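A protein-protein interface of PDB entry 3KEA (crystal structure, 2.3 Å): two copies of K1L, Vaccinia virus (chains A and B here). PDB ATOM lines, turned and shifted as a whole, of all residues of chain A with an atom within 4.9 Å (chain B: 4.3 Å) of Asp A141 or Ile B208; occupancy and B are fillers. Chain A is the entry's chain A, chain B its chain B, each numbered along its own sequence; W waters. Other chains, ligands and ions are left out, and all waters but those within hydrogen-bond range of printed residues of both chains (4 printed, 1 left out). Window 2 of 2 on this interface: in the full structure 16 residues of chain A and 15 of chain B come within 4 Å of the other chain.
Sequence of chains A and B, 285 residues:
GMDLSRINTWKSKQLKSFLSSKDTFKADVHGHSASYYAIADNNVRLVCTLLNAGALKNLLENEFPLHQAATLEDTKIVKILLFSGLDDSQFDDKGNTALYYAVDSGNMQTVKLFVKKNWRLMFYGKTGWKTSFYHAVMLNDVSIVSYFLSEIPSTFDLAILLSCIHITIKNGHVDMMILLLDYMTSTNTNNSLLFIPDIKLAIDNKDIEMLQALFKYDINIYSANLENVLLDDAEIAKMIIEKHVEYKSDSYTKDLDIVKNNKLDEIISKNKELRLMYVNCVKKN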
ATOM      1  N   ALA A 136     -19.537 -23.391  10.630  1.00  0.00           N
ATOM      2  CA  ALA A 136     -18.785 -22.120  10.502  1.00  0.00           C
ATOM      3  C   ALA A 136     -18.185 -21.906   9.118  1.00  0.00           C
ATOM      4  O   ALA A 136     -18.205 -20.794   8.592  1.00  0.00           O
ATOM      5  CB  ALA A 136     -17.673 -22.019  11.562  1.00  0.00           C
ATOM      6  N   VAL A 137     -17.631 -22.973   8.549  1.00  0.00           N
ATOM      7  CA  VAL A 137     -17.139 -22.978   7.184  1.00  0.00           C
ATOM      8  C   VAL A 137     -18.283 -22.734   6.209  1.00  0.00           C
ATOM      9  O   VAL A 137     -18.184 -21.879   5.347  1.00  0.00           O
ATOM     10  CB  VAL A 137     -16.417 -24.323   6.826  1.00  0.00           C
ATOM     11  CG1 VAL A 137     -16.032 -24.357   5.384  1.00  0.00           C
ATOM     12  CG2 VAL A 137     -15.165 -24.509   7.680  1.00  0.00           C
ATOM     13  N   LEU A 139     -20.967 -21.227   6.606  1.00  0.00           N
ATOM     14  CA  LEU A 139     -21.538 -19.885   6.814  1.00  0.00           C
ATOM     15  C   LEU A 139     -20.599 -18.812   6.304  1.00  0.00           C
ATOM     16  O   LEU A 139     -20.940 -17.632   6.306  1.00  0.00           O
ATOM     17  CB  LEU A 139     -21.824 -19.611   8.302  1.00  0.00           C
ATOM     18  CG  LEU A 139     -23.045 -20.200   9.008  1.00  0.00           C
ATOM     19  CD1 LEU A 139     -23.130 -19.674  10.435  1.00  0.00           C
ATOM     20  CD2 LEU A 139     -24.335 -19.910   8.278  1.00  0.00           C
ATOM     21  N   ASN A 140     -19.425 -19.242   5.849  1.00  0.00           N
ATOM     22  CA  ASN A 140     -18.296 -18.362   5.567  1.00  0.00           C
ATOM     23  C   ASN A 140     -18.030 -17.425   6.733  1.00  0.00           C
ATOM     24  O   ASN A 140     -17.817 -16.246   6.530  1.00  0.00           O
ATOM     25  CB  ASN A 140     -18.464 -17.577   4.256  1.00  0.00           C
ATOM     26  CG  ASN A 140     -17.150 -16.940   3.758  1.00  0.00           C
ATOM     27  OD1 ASN A 140     -16.044 -17.372   4.112  1.00  0.00           O
ATOM     28  ND2 ASN A 140     -17.274 -15.909   2.914  1.00  0.00           N
ATOM     29  N   ASP A 141     -18.043 -17.949   7.958  1.00  0.00           N
ATOM     30  CA  ASP A 141     -17.686 -17.113   9.110  1.00  0.00           C
ATOM     31  C   ASP A 141     -16.194 -17.220   9.427  1.00  0.00           C
ATOM     32  O   ASP A 141     -15.775 -18.016  10.274  1.00  0.00           O
ATOM     33  CB  ASP A 141     -18.507 -17.419  10.345  1.00  0.00           C
ATOM     34  CG  ASP A 141     -18.270 -16.398  11.438  1.00  0.00           C
ATOM     35  OD1 ASP A 141     -17.171 -15.779  11.440  1.00  0.00           O
ATOM     36  OD2 ASP A 141     -19.174 -16.200  12.290  1.00  0.00           O
ATOM     37  N   VAL A 142     -15.408 -16.390   8.746  1.00  0.00           N
ATOM     38  CA  VAL A 142     -13.951 -16.502   8.769  1.00  0.00           C
ATOM     39  C   VAL A 142     -13.373 -16.275  10.159  1.00  0.00           C
ATOM     40  O   VAL A 142     -12.396 -16.949  10.507  1.00  0.00           O
ATOM     41  CB  VAL A 142     -13.205 -15.623   7.680  1.00  0.00           C
ATOM     42  CG1 VAL A 142     -13.341 -16.219   6.329  1.00  0.00           C
ATOM     43  CG2 VAL A 142     -13.714 -14.216   7.670  1.00  0.00           C
ATOM     44  N   SER A 143     -13.984 -15.382  10.947  1.00  0.00           N
ATOM     45  CA  SER A 143     -13.578 -15.148  12.344  1.00  0.00           C
ATOM     46  C   SER A 143     -13.701 -16.376  13.218  1.00  0.00           C
ATOM     47  O   SER A 143     -12.785 -16.687  13.969  1.00  0.00           O
ATOM     48  CB  SER A 143     -14.406 -14.032  13.023  1.00  0.00           C
ATOM     49  OG  SER A 143     -14.332 -12.834  12.287  1.00  0.00           O
ATOM     50  N   ILE A 144     -14.855 -17.038  13.157  1.00  0.00           N
ATOM     51  CA  ILE A 144     -15.040 -18.240  13.963  1.00  0.00           C
ATOM     52  C   ILE A 144     -14.040 -19.334  13.551  1.00  0.00           C
ATOM     53  O   ILE A 144     -13.368 -19.915  14.403  1.00  0.00           O
ATOM     54  CB  ILE A 144     -16.493 -18.710  14.017  1.00  0.00           C
ATOM     55  CG1 ILE A 144     -17.344 -17.654  14.720  1.00  0.00           C
ATOM     56  CG2 ILE A 144     -16.576 -20.045  14.747  1.00  0.00           C
ATOM     57  CD1 ILE A 144     -18.816 -18.069  14.916  1.00  0.00           C
ATOM     58  N   VAL A 145     -13.903 -19.574  12.251  1.00  0.00           N
ATOM     59  CA  VAL A 145     -12.983 -20.611  11.768  1.00  0.00           C
ATOM     60  C   VAL A 145     -11.509 -20.277  12.085  1.00  0.00           C
ATOM     61  O   VAL A 145     -10.731 -21.117  12.498  1.00  0.00           O
ATOM     62  CB  VAL A 145     -13.168 -20.855  10.285  1.00  0.00           C
ATOM     63  CG1 VAL A 145     -12.164 -21.909   9.790  1.00  0.00           C
ATOM     64  CG2 VAL A 145     -14.589 -21.300  10.043  1.00  0.00           C
ATOM     65  N   MET A 176     -11.687 -17.914   3.240  1.00  0.00           N
ATOM     66  CA  MET A 176     -11.869 -19.160   3.909  1.00  0.00           C
ATOM     67  C   MET A 176     -10.867 -20.194   3.411  1.00  0.00           C
ATOM     68  O   MET A 176     -10.187 -20.803   4.226  1.00  0.00           O
ATOM     69  CB  MET A 176     -13.300 -19.678   3.734  1.00  0.00           C
ATOM     70  CG  MET A 176     -13.588 -20.947   4.556  1.00  0.00           C
ATOM     71  SD  MET A 176     -13.377 -20.625   6.484  1.00  0.00           S
ATOM     72  CE  MET A 176     -15.055 -19.676   6.670  1.00  0.00           C
ATOM     73  N   LYS B 206     -26.763 -16.172   3.524  1.00  0.00           N
ATOM     74  CA  LYS B 206     -26.096 -16.059   4.819  1.00  0.00           C
ATOM     75  C   LYS B 206     -24.578 -16.277   4.693  1.00  0.00           C
ATOM     76  O   LYS B 206     -24.032 -17.214   5.269  1.00  0.00           O
ATOM     77  CB  LYS B 206     -26.707 -17.028   5.833  1.00  0.00           C
ATOM     78  CG  LYS B 206     -26.753 -16.418   7.180  1.00  0.00           C
ATOM     79  CD  LYS B 206     -26.975 -17.407   8.282  1.00  0.00           C
ATOM     80  CE  LYS B 206     -26.550 -16.794   9.604  1.00  0.00           C
ATOM     81  NZ  LYS B 206     -27.009 -17.667  10.719  1.00  0.00           N
ATOM     82  N   ASP B 207     -23.922 -15.420   3.909  1.00  0.00           N
ATOM     83  CA  ASP B 207     -22.477 -15.393   3.788  1.00  0.00           C
ATOM     84  C   ASP B 207     -22.034 -14.362   4.795  1.00  0.00           C
ATOM     85  O   ASP B 207     -22.172 -13.156   4.564  1.00  0.00           O
ATOM     86  CB  ASP B 207     -22.107 -14.989   2.357  1.00  0.00           C
ATOM     87  CG  ASP B 207     -20.602 -14.933   2.102  1.00  0.00           C
ATOM     88  OD1 ASP B 207     -20.196 -15.216   0.956  1.00  0.00           O
ATOM     89  OD2 ASP B 207     -19.826 -14.558   3.003  1.00  0.00           O
ATOM     90  N   ILE B 208     -21.513 -14.829   5.923  1.00  0.00           N
ATOM     91  CA  ILE B 208     -21.166 -13.937   7.031  1.00  0.00           C
ATOM     92  C   ILE B 208     -20.080 -12.917   6.672  1.00  0.00           C
ATOM     93  O   ILE B 208     -20.218 -11.756   7.029  1.00  0.00           O
ATOM     94  CB  ILE B 208     -20.799 -14.709   8.343  1.00  0.00           C
ATOM     95  CG1 ILE B 208     -21.998 -15.474   8.896  1.00  0.00           C
ATOM     96  CG2 ILE B 208     -20.240 -13.756   9.403  1.00  0.00           C
ATOM     97  CD1 ILE B 208     -23.252 -14.611   9.195  1.00  0.00           C
ATOM     98  N   GLU B 209     -19.026 -13.333   5.962  1.00  0.00           N
ATOM     99  CA  GLU B 209     -17.977 -12.389   5.555  1.00  0.00           C
ATOM    100  C   GLU B 209     -18.500 -11.320   4.577  1.00  0.00           C
ATOM    101  O   GLU B 209     -18.131 -10.140   4.687  1.00  0.00           O
ATOM    102  CB  GLU B 209     -16.722 -13.084   4.994  1.00  0.00           C
ATOM    103  CG  GLU B 209     -15.473 -12.176   5.057  1.00  0.00           C
ATOM    104  CD  GLU B 209     -14.308 -12.633   4.198  1.00  0.00           C
ATOM    105  OE1 GLU B 209     -13.166 -12.147   4.416  1.00  0.00           O
ATOM    106  OE2 GLU B 209     -14.498 -13.477   3.303  1.00  0.00           O
ATOM    107  N   MET B 210     -19.369 -11.737   3.646  1.00  0.00           N
ATOM    108  CA  MET B 210     -20.013 -10.820   2.692  1.00  0.00           C
ATOM    109  C   MET B 210     -20.854  -9.790   3.427  1.00  0.00           C
ATOM    110  O   MET B 210     -20.658  -8.577   3.239  1.00  0.00           O
ATOM    111  CB  MET B 210     -20.872 -11.578   1.663  1.00  0.00           C
ATOM    112  CG  MET B 210     -21.628 -10.702   0.640  1.00  0.00           C
ATOM    113  SD  MET B 210     -20.461  -9.772  -0.644  1.00  0.00           S
ATOM    114  CE  MET B 210     -20.191 -11.245  -1.898  1.00  0.00           C
ATOM    115  N   LEU B 211     -21.778 -10.268   4.266  1.00  0.00           N
ATOM    116  CA  LEU B 211     -22.627  -9.379   5.081  1.00  0.00           C
ATOM    117  C   LEU B 211     -21.840  -8.427   5.989  1.00  0.00           C
ATOM    118  O   LEU B 211     -22.154  -7.244   6.067  1.00  0.00           O
ATOM    119  CB  LEU B 211     -23.612 -10.196   5.902  1.00  0.00           C
ATOM    120  CG  LEU B 211     -24.719 -10.895   5.104  1.00  0.00           C
ATOM    121  CD1 LEU B 211     -25.401 -11.900   5.996  1.00  0.00           C
ATOM    122  CD2 LEU B 211     -25.718  -9.890   4.545  1.00  0.00           C
ATOM    123  N   GLN B 212     -20.827  -8.939   6.673  1.00  0.00           N
ATOM    124  CA  GLN B 212     -19.983  -8.102   7.523  1.00  0.00           C
ATOM    125  C   GLN B 212     -19.316  -6.977   6.732  1.00  0.00           C
ATOM    126  O   GLN B 212     -19.199  -5.858   7.225  1.00  0.00           O
ATOM    127  CB  GLN B 212     -18.919  -8.958   8.229  1.00  0.00           C
ATOM    128  CG  GLN B 212     -19.418  -9.601   9.495  1.00  0.00           C
ATOM    129  CD  GLN B 212     -18.473 -10.644  10.077  1.00  0.00           C
ATOM    130  OE1 GLN B 212     -17.516 -11.110   9.430  1.00  0.00           O
ATOM    131  NE2 GLN B 212     -18.770 -11.053  11.294  1.00  0.00           N
ATOM    132  N   GLU B 235     -29.023 -13.626  13.975  1.00  0.00           N
ATOM    133  CA  GLU B 235     -27.673 -13.112  13.755  1.00  0.00           C
ATOM    134  C   GLU B 235     -27.725 -11.957  12.739  1.00  0.00           C
ATOM    135  O   GLU B 235     -27.081 -10.923  12.931  1.00  0.00           O
ATOM    136  CB  GLU B 235     -26.742 -14.219  13.268  1.00  0.00           C
ATOM    137  CG  GLU B 235     -25.309 -13.778  12.988  1.00  0.00           C
ATOM    138  CD  GLU B 235     -24.393 -14.939  12.636  1.00  0.00           C
ATOM    139  OE1 GLU B 235     -23.172 -14.828  12.862  1.00  0.00           O
ATOM    140  OE2 GLU B 235     -24.885 -15.974  12.139  1.00  0.00           O
HETATM  141  O   HOH W   1     -19.922 -14.324  13.932  1.00  0.00           O
HETATM  142  O   HOH W   2     -21.853 -16.888  12.337  1.00  0.00           O
HETATM  143  O   HOH W   3     -16.318 -13.615   9.714  1.00  0.00           O
HETATM  144  O   HOH W   4     -14.175 -16.500   2.629  1.00  0.00           O
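Among the printed residues, merely in contact across the chains: Leu A139 with Asp B207 (3.7 Å), Val A142 with Glu B209 (3.8 Å), Asn A140 with Ile B208 (3.8 Å) and Asp A141 with Ile B208 (3.9 Å).
No position is printed for both chains.
Of the 8 pairs that touch across the chains among the printed residues, none has its exchanged pair printed and touching as well.
The side-chain carboxylate (OD2) of Asp B207 is in hydrogen-bond range of the backbone NH (N) of Glu B209 (3.3 Å).
OD1 of Asp A141 lies within hydrogen-bond range of N of Ser A143 (3.2 Å).
The side-chain carboxylate (OD2) of Asp B207 is in hydrogen-bond range of the backbone NH (N) of Met B210.
NZ of Lys B206 is in salt-bridge range of OE2 of Glu B235 (3.1 Å).
The backbone NH (N) of Asp A141 sits at hydrogen-bond distance from the backbone carbonyl oxygen (O) of Ala A136.
N of Ile A144 is in hydrogen-bond range of OD1 of Asp A141 (3.1 Å).
Of the 8 printed residues of chain B, 4 touch a printed residue of chain A.
Hydrophobic or aromatic side chains of chain B within 4 Å of the printed part of chain A: Ile B208.
Printed residues of chain A that touch a printed residue of chain B: Leu A139, Asn A140, Asp A141 and Val A142.
Hydrophobic or aromatic side chains of chain A that line the printed part of chain B: Leu A139 and Val A142.
Among the printed residues, 8 pairs touch across the chains.
Among the printed residues, no Asp or Glu carboxylate lies within 4 Å of a Lys or Arg side-chain nitrogen of the other chain.
Water W2 lies within hydrogen-bond range of the side-chain carboxylate (OE1) of Glu B235 and the side-chain carboxylate (OD2) of Asp A141.
Water W4 lies within hydrogen-bond range of OD1 of Asn A140 (2.5 Å), N of Met A176 (2.9 Å) and OE2 of Glu B209 (3.1 Å).
Water W1 bridges OD2 of Asp A141 and OE1 of Glu B235.
Water W3 lies within hydrogen-bond range of OE1 of Gln B212 (2.8 Å), OD1 of Asp A141 (2.9 Å), N of Val A142 (3.1 Å) and N of Ser A143 (3.2 Å).
Of chain B, only Ile B208 comes within 4 Å of Asp A141.
Of chain A, only Leu A139 (2.9 Å), Asn A140 (3.8 Å) and Asp A141 (3.9 Å) come within 4 Å of Ile B208.
Of the printed residues of chain A, Asp B207 touches Leu A139 and Asn A140.
Printed residues of chain B within 4 Å of Val A142: Glu B209 (3.8 Å).
Of the printed residues of chain A, Glu B209 touches Asn A140 and Val A142.
Of the printed residues of chain A, Lys B206 touches Leu A139 (3.3 Å).
Ile A144 touches none of the printed residues of chain B.
Met B210 touches none of the printed residues of chain A.
The nearest printed residue of chain B that does not touch Asp A141 is Glu B235 (4.3 Å).
The nearest printed residue of chain A that does not touch Ile B208 is Val A142 (5.5 Å).
The nearest printed residue of chain A that does not touch Asp B207 is Asp A141 (6.2 Å).
The side-chain amide nitrogen (ND2) of Asn A140 sits at hydrogen-bond distance from the side-chain carboxylate (OD2) of Asp B207, 2.9 Å away.
N of Glu B209 sits at hydrogen-bond distance from O of Asn A140 (3.2 Å).
The backbone carbonyl oxygen of Leu A139 lies close to the backbone carbonyl oxygen of Lys B206, at 3.3 Å.
O of Leu A139 lies within hydrogen-bond range of N of Ile B208 (2.9 Å).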
